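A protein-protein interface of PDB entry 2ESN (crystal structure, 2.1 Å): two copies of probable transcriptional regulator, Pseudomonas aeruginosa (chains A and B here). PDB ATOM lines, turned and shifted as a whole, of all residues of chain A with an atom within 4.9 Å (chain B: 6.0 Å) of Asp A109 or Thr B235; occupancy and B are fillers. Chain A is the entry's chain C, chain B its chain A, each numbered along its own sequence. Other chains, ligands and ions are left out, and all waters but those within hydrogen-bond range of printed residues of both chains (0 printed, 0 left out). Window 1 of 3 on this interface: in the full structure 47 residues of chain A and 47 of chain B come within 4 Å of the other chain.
Printed residues of chain A within 4 Å of Thr B235: Asp A109 (3.6 Å).
Of the printed residues of chain B, Ala A112 touches Ala B238 (3.9 Å).
Of the printed residues of chain B, Thr A235 touches Asp B109 (3.5 Å).
Printed residues of chain B within 4 Å of Ala A238: Asp B109 (3.8 Å) and Leu B237 (3.7 Å).
Of the printed residues of chain A, Ala B238 touches Asp A109, Ala A112, Phe A113 and Leu A237.
Of the printed residues of chain B, Phe A113 touches Ala B238 (3.8 Å).
Ala A107 touches none of the printed residues of chain B.
The nearest residue of chain A that does not touch Thr B235 is Ala A112 (4.1 Å).
Printed residues of chain B that touch a printed residue of chain A: Asp B109, Thr B235, Leu B237 and Ala B238.
Hydrophobic or aromatic side chains of chain B that line the printed part of chain A: Leu B237 and Ala B238.
Of the 12 printed residues of chain A, 6 touch a printed residue of chain B.
Among the printed residues, 9 pairs touch across the chains.
Asp A109 touches Thr B235, and with the chains exchanged Thr A235 touches Asp B109.
Asp A109 touches Ala B238, and with the chains exchanged Ala A238 touches Asp B109.
Leu A237 touches its own counterpart, Leu B237.
Leu A237 touches Ala B238, and with the chains exchanged Ala A238 touches Leu B237.
Of the 9 pairs that touch across the chains among the printed residues, 7 have their exchanged pair printed and touching as well.
OD1 of Asp B109 lies within hydrogen-bond range of N of Val B236, 3.1 Å away.
The side-chain hydroxyl (OG1) of Thr B235 is in hydrogen-bond range of the backbone NH (N) of Ala B238 (3.3 Å).
The side-chain hydroxyl of Thr A235 sits at hydrogen-bond distance from the side-chain carboxylate of Asp A109.
The backbone NH of Val A236 sits at hydrogen-bond distance from the side-chain carboxylate of Asp A109 (3.1 Å).
The side-chain carboxylate (OD2) of Asp A109 sits at hydrogen-bond distance from the backbone NH (N) of Leu A237, 3.1 Å away.
The side-chain hydroxyl (OG1) of Thr A235 is in hydrogen-bond range of the backbone NH (N) of Ala A238, 3.3 Å away.
Asp A109 touches Thr B235.
O of Asp A109 touches CB of Ala B238 (3.8 Å).
CB of Ala A112 touches CB of Ala B238, 3.9 Å away.
N of Phe A113 touches CB of Ala B238, 3.8 Å away.
Thr A235 touches Asp B109 (OG1 to CB, 3.5 Å).
Leu A237 touches Leu B237.
Leu A237 touches Ala B238 (CD1 to N, 3.6 Å).
Ala A238 touches Asp B109.
Ala A238 touches Leu B237.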
ATOM      1  N   ALA A 107      -1.797 -25.980 -27.245  1.00  0.00           N
ATOM      2  CA  ALA A 107      -2.716 -25.132 -26.469  1.00  0.00           C
ATOM      3  C   ALA A 107      -3.077 -25.800 -25.177  1.00  0.00           C
ATOM      4  O   ALA A 107      -2.588 -26.896 -24.888  1.00  0.00           O
ATOM      5  CB  ALA A 107      -3.928 -24.776 -27.284  1.00  0.00           C
ATOM      6  N   THR A 108      -3.963 -25.152 -24.403  1.00  0.00           N
ATOM      7  CA  THR A 108      -4.468 -25.639 -23.137  1.00  0.00           C
ATOM      8  C   THR A 108      -5.964 -25.424 -23.245  1.00  0.00           C
ATOM      9  O   THR A 108      -6.441 -24.785 -24.189  1.00  0.00           O
ATOM     10  CB  THR A 108      -3.947 -24.756 -21.936  1.00  0.00           C
ATOM     11  OG1 THR A 108      -4.386 -23.398 -22.137  1.00  0.00           O
ATOM     12  CG2 THR A 108      -2.442 -24.780 -21.906  1.00  0.00           C
ATOM     13  N   ASP A 109      -6.739 -25.948 -22.306  1.00  0.00           N
ATOM     14  CA  ASP A 109      -8.165 -25.641 -22.318  1.00  0.00           C
ATOM     15  C   ASP A 109      -8.583 -24.126 -22.239  1.00  0.00           C
ATOM     16  O   ASP A 109      -9.493 -23.704 -22.889  1.00  0.00           O
ATOM     17  CB  ASP A 109      -8.917 -26.521 -21.300  1.00  0.00           C
ATOM     18  CG  ASP A 109      -8.868 -25.987 -19.895  1.00  0.00           C
ATOM     19  OD1 ASP A 109      -7.817 -25.427 -19.474  1.00  0.00           O
ATOM     20  OD2 ASP A 109      -9.925 -26.136 -19.224  1.00  0.00           O
ATOM     21  N   TYR A 110      -7.891 -23.355 -21.455  1.00  0.00           N
ATOM     22  CA  TYR A 110      -8.107 -21.942 -21.354  1.00  0.00           C
ATOM     23  C   TYR A 110      -7.804 -21.206 -22.655  1.00  0.00           C
ATOM     24  O   TYR A 110      -8.626 -20.459 -23.124  1.00  0.00           O
ATOM     25  CB  TYR A 110      -7.199 -21.366 -20.240  1.00  0.00           C
ATOM     26  CG  TYR A 110      -7.416 -19.874 -20.199  1.00  0.00           C
ATOM     27  CD1 TYR A 110      -8.716 -19.364 -20.176  1.00  0.00           C
ATOM     28  CD2 TYR A 110      -6.345 -18.957 -20.224  1.00  0.00           C
ATOM     29  CE1 TYR A 110      -8.988 -17.966 -20.183  1.00  0.00           C
ATOM     30  CE2 TYR A 110      -6.645 -17.498 -20.203  1.00  0.00           C
ATOM     31  CZ  TYR A 110      -7.948 -17.076 -20.208  1.00  0.00           C
ATOM     32  OH  TYR A 110      -8.296 -15.741 -20.237  1.00  0.00           O
ATOM     33  N   THR A 111      -6.667 -21.478 -23.304  1.00  0.00           N
ATOM     34  CA  THR A 111      -6.470 -20.823 -24.619  1.00  0.00           C
ATOM     35  C   THR A 111      -7.418 -21.265 -25.682  1.00  0.00           C
ATOM     36  O   THR A 111      -7.848 -20.471 -26.502  1.00  0.00           O
ATOM     37  CB  THR A 111      -4.979 -20.849 -25.044  1.00  0.00           C
ATOM     38  OG1 THR A 111      -4.563 -22.238 -25.051  1.00  0.00           O
ATOM     39  CG2 THR A 111      -4.138 -20.084 -23.985  1.00  0.00           C
ATOM     40  N   ALA A 112      -7.830 -22.536 -25.650  1.00  0.00           N
ATOM     41  CA  ALA A 112      -8.793 -23.026 -26.617  1.00  0.00           C
ATOM     42  C   ALA A 112     -10.091 -22.279 -26.356  1.00  0.00           C
ATOM     43  O   ALA A 112     -10.734 -21.770 -27.279  1.00  0.00           O
ATOM     44  CB  ALA A 112      -8.997 -24.587 -26.366  1.00  0.00           C
ATOM     45  N   PHE A 113     -10.492 -22.231 -25.089  1.00  0.00           N
ATOM     46  CA  PHE A 113     -11.727 -21.506 -24.689  1.00  0.00           C
ATOM     47  C   PHE A 113     -11.721 -20.004 -25.101  1.00  0.00           C
ATOM     48  O   PHE A 113     -12.722 -19.457 -25.522  1.00  0.00           O
ATOM     49  CB  PHE A 113     -11.902 -21.632 -23.176  1.00  0.00           C
ATOM     50  CG  PHE A 113     -12.837 -20.562 -22.566  1.00  0.00           C
ATOM     51  CD1 PHE A 113     -14.234 -20.735 -22.563  1.00  0.00           C
ATOM     52  CD2 PHE A 113     -12.308 -19.414 -21.986  1.00  0.00           C
ATOM     53  CE1 PHE A 113     -15.081 -19.763 -22.026  1.00  0.00           C
ATOM     54  CE2 PHE A 113     -13.159 -18.400 -21.440  1.00  0.00           C
ATOM     55  CZ  PHE A 113     -14.558 -18.585 -21.453  1.00  0.00           C
ATOM     56  N   PRO A 234      -4.717 -29.819 -14.840  1.00  0.00           N
ATOM     57  CA  PRO A 234      -4.300 -29.016 -16.017  1.00  0.00           C
ATOM     58  C   PRO A 234      -5.334 -28.114 -16.619  1.00  0.00           C
ATOM     59  O   PRO A 234      -5.014 -27.239 -17.429  1.00  0.00           O
ATOM     60  CB  PRO A 234      -3.866 -30.088 -17.088  1.00  0.00           C
ATOM     61  CG  PRO A 234      -3.973 -31.380 -16.418  1.00  0.00           C
ATOM     62  CD  PRO A 234      -4.877 -31.242 -15.196  1.00  0.00           C
ATOM     63  N   THR A 235      -6.575 -28.256 -16.172  1.00  0.00           N
ATOM     64  CA  THR A 235      -7.701 -27.680 -16.858  1.00  0.00           C
ATOM     65  C   THR A 235      -8.418 -26.636 -15.977  1.00  0.00           C
ATOM     66  O   THR A 235      -8.863 -26.951 -14.878  1.00  0.00           O
ATOM     67  CB  THR A 235      -8.724 -28.850 -17.184  1.00  0.00           C
ATOM     68  OG1 THR A 235     -10.031 -28.272 -17.327  1.00  0.00           O
ATOM     69  CG2 THR A 235      -8.744 -29.849 -15.995  1.00  0.00           C
ATOM     70  N   VAL A 236      -8.500 -25.409 -16.455  1.00  0.00           N
ATOM     71  CA  VAL A 236      -9.130 -24.305 -15.689  1.00  0.00           C
ATOM     72  C   VAL A 236     -10.660 -24.432 -15.657  1.00  0.00           C
ATOM     73  O   VAL A 236     -11.266 -24.125 -14.671  1.00  0.00           O
ATOM     74  CB  VAL A 236      -8.743 -22.838 -16.189  1.00  0.00           C
ATOM     75  CG1 VAL A 236      -9.340 -22.446 -17.529  1.00  0.00           C
ATOM     76  CG2 VAL A 236      -9.238 -21.810 -15.168  1.00  0.00           C
ATOM     77  N   LEU A 237     -11.281 -24.833 -16.768  1.00  0.00           N
ATOM     78  CA  LEU A 237     -12.741 -24.884 -16.765  1.00  0.00           C
ATOM     79  C   LEU A 237     -13.276 -25.918 -15.784  1.00  0.00           C
ATOM     80  O   LEU A 237     -14.285 -25.666 -15.113  1.00  0.00           O
ATOM     81  CB  LEU A 237     -13.298 -25.035 -18.176  1.00  0.00           C
ATOM     82  CG  LEU A 237     -12.743 -24.009 -19.195  1.00  0.00           C
ATOM     83  CD1 LEU A 237     -13.062 -24.460 -20.632  1.00  0.00           C
ATOM     84  CD2 LEU A 237     -13.255 -22.670 -18.907  1.00  0.00           C
ATOM     85  N   ALA A 238     -12.540 -27.026 -15.637  1.00  0.00           N
ATOM     86  CA  ALA A 238     -12.895 -28.054 -14.673  1.00  0.00           C
ATOM     87  C   ALA A 238     -12.572 -27.536 -13.299  1.00  0.00           C
ATOM     88  O   ALA A 238     -13.361 -27.722 -12.380  1.00  0.00           O
ATOM     89  CB  ALA A 238     -12.113 -29.395 -14.975  1.00  0.00           C
ATOM     90  N   ASP B 109      -9.957 -33.334 -19.377  1.00  0.00           N
ATOM     91  CA  ASP B 109     -10.778 -32.315 -18.690  1.00  0.00           C
ATOM     92  C   ASP B 109     -12.139 -32.815 -18.317  1.00  0.00           C
ATOM     93  O   ASP B 109     -12.702 -32.372 -17.326  1.00  0.00           O
ATOM     94  CB  ASP B 109     -10.894 -30.965 -19.427  1.00  0.00           C
ATOM     95  CG  ASP B 109     -11.813 -31.008 -20.569  1.00  0.00           C
ATOM     96  OD1 ASP B 109     -11.870 -32.073 -21.285  1.00  0.00           O
ATOM     97  OD2 ASP B 109     -12.444 -29.960 -20.800  1.00  0.00           O
ATOM     98  N   VAL B 206     -13.665 -33.868 -30.044  1.00  0.00           N
ATOM     99  CA  VAL B 206     -12.764 -33.918 -28.896  1.00  0.00           C
ATOM    100  C   VAL B 206     -11.853 -35.123 -29.049  1.00  0.00           C
ATOM    101  O   VAL B 206     -12.345 -36.265 -29.228  1.00  0.00           O
ATOM    102  CB  VAL B 206     -13.574 -34.037 -27.574  1.00  0.00           C
ATOM    103  CG1 VAL B 206     -12.676 -34.175 -26.421  1.00  0.00           C
ATOM    104  CG2 VAL B 206     -14.510 -32.801 -27.393  1.00  0.00           C
ATOM    105  N   THR B 207     -10.548 -34.828 -29.010  1.00  0.00           N
ATOM    106  CA  THR B 207      -9.443 -35.798 -29.137  1.00  0.00           C
ATOM    107  C   THR B 207      -8.575 -35.718 -27.902  1.00  0.00           C
ATOM    108  O   THR B 207      -7.476 -35.108 -27.916  1.00  0.00           O
ATOM    109  CB  THR B 207      -8.625 -35.474 -30.402  1.00  0.00           C
ATOM    110  OG1 THR B 207      -8.285 -34.072 -30.399  1.00  0.00           O
ATOM    111  CG2 THR B 207      -9.464 -35.723 -31.622  1.00  0.00           C
ATOM    112  N   PRO B 208      -9.029 -36.332 -26.807  1.00  0.00           N
ATOM    113  CA  PRO B 208      -8.334 -35.948 -25.578  1.00  0.00           C
ATOM    114  C   PRO B 208      -6.875 -36.418 -25.490  1.00  0.00           C
ATOM    115  O   PRO B 208      -6.172 -35.942 -24.608  1.00  0.00           O
ATOM    116  CB  PRO B 208      -9.147 -36.626 -24.464  1.00  0.00           C
ATOM    117  CG  PRO B 208     -10.274 -37.409 -25.146  1.00  0.00           C
ATOM    118  CD  PRO B 208     -10.063 -37.375 -26.627  1.00  0.00           C
ATOM    119  N   LEU B 233      -9.897 -30.830 -30.709  1.00  0.00           N
ATOM    120  CA  LEU B 233      -9.201 -30.228 -29.537  1.00  0.00           C
ATOM    121  C   LEU B 233      -9.404 -31.228 -28.431  1.00  0.00           C
ATOM    122  O   LEU B 233     -10.307 -31.989 -28.511  1.00  0.00           O
ATOM    123  CB  LEU B 233      -9.872 -28.863 -29.078  1.00  0.00           C
ATOM    124  CG  LEU B 233     -11.390 -28.834 -28.595  1.00  0.00           C
ATOM    125  CD1 LEU B 233     -11.646 -27.386 -28.192  1.00  0.00           C
ATOM    126  CD2 LEU B 233     -12.419 -29.154 -29.773  1.00  0.00           C
ATOM    127  N   PRO B 234      -8.553 -31.216 -27.400  1.00  0.00           N
ATOM    128  CA  PRO B 234      -8.608 -32.235 -26.411  1.00  0.00           C
ATOM    129  C   PRO B 234      -9.618 -32.027 -25.296  1.00  0.00           C
ATOM    130  O   PRO B 234      -9.770 -32.902 -24.437  1.00  0.00           O
ATOM    131  CB  PRO B 234      -7.156 -32.294 -25.863  1.00  0.00           C
ATOM    132  CG  PRO B 234      -6.348 -31.204 -26.647  1.00  0.00           C
ATOM    133  CD  PRO B 234      -7.367 -30.313 -27.256  1.00  0.00           C
ATOM    134  N   THR B 235     -10.329 -30.901 -25.310  1.00  0.00           N
ATOM    135  CA  THR B 235     -11.055 -30.495 -24.128  1.00  0.00           C
ATOM    136  C   THR B 235     -12.542 -30.341 -24.433  1.00  0.00           C
ATOM    137  O   THR B 235     -12.904 -29.566 -25.288  1.00  0.00           O
ATOM    138  CB  THR B 235     -10.439 -29.108 -23.584  1.00  0.00           C
ATOM    139  OG1 THR B 235     -11.463 -28.433 -22.885  1.00  0.00           O
ATOM    140  CG2 THR B 235     -10.034 -28.182 -24.761  1.00  0.00           C
ATOM    141  N   VAL B 236     -13.403 -31.102 -23.746  1.00  0.00           N
ATOM    142  CA  VAL B 236     -14.837 -31.043 -23.971  1.00  0.00           C
ATOM    143  C   VAL B 236     -15.463 -29.678 -23.558  1.00  0.00           C
ATOM    144  O   VAL B 236     -16.365 -29.177 -24.204  1.00  0.00           O
ATOM    145  CB  VAL B 236     -15.574 -32.161 -23.215  1.00  0.00           C
ATOM    146  CG1 VAL B 236     -16.952 -32.333 -23.876  1.00  0.00           C
ATOM    147  CG2 VAL B 236     -14.875 -33.473 -23.488  1.00  0.00           C
ATOM    148  N   LEU B 237     -14.997 -29.131 -22.462  1.00  0.00           N
ATOM    149  CA  LEU B 237     -15.627 -27.953 -21.858  1.00  0.00           C
ATOM    150  C   LEU B 237     -15.395 -26.742 -22.763  1.00  0.00           C
ATOM    151  O   LEU B 237     -16.335 -26.015 -23.056  1.00  0.00           O
ATOM    152  CB  LEU B 237     -15.104 -27.765 -20.413  1.00  0.00           C
ATOM    153  CG  LEU B 237     -15.433 -28.914 -19.388  1.00  0.00           C
ATOM    154  CD1 LEU B 237     -15.045 -28.488 -17.932  1.00  0.00           C
ATOM    155  CD2 LEU B 237     -16.901 -29.413 -19.427  1.00  0.00           C
ATOM    156  N   ALA B 238     -14.180 -26.558 -23.277  1.00  0.00           N
ATOM    157  CA  ALA B 238     -13.958 -25.535 -24.325  1.00  0.00           C
ATOM    158  C   ALA B 238     -14.747 -25.851 -25.573  1.00  0.00           C
ATOM    159  O   ALA B 238     -15.290 -24.945 -26.229  1.00  0.00           O
ATOM    160  CB  ALA B 238     -12.422 -25.428 -24.632  1.00  0.00           C
ATOM    161  N   ALA B 239     -14.839 -27.154 -25.924  1.00  0.00           N
ATOM    162  CA  ALA B 239     -15.533 -27.528 -27.140  1.00  0.00           C
ATOM    163  C   ALA B 239     -16.994 -27.079 -27.125  1.00  0.00           C
ATOM    164  O   ALA B 239     -17.511 -26.708 -28.157  1.00  0.00           O
ATOM    165  CB  ALA B 239     -15.406 -29.052 -27.464  1.00  0.00           C
ATOM    166  N   LEU B 240     -17.630 -27.094 -25.952  1.00  0.00           N
ATOM    167  CA  LEU B 240     -19.065 -26.712 -25.773  1.00  0.00           C
ATOM    168  C   LEU B 240     -19.192 -25.180 -25.986  1.00  0.00           C
ATOM    169  O   LEU B 240     -20.147 -24.729 -26.585  1.00  0.00           O
ATOM    170  CB  LEU B 240     -19.452 -27.075 -24.329  1.00  0.00           C
ATOM    171  CG  LEU B 240     -19.658 -28.640 -24.211  1.00  0.00           C
ATOM    172  CD1 LEU B 240     -19.633 -29.221 -22.736  1.00  0.00           C
ATOM    173  CD2 LEU B 240     -20.992 -28.941 -24.862  1.00  0.00           C
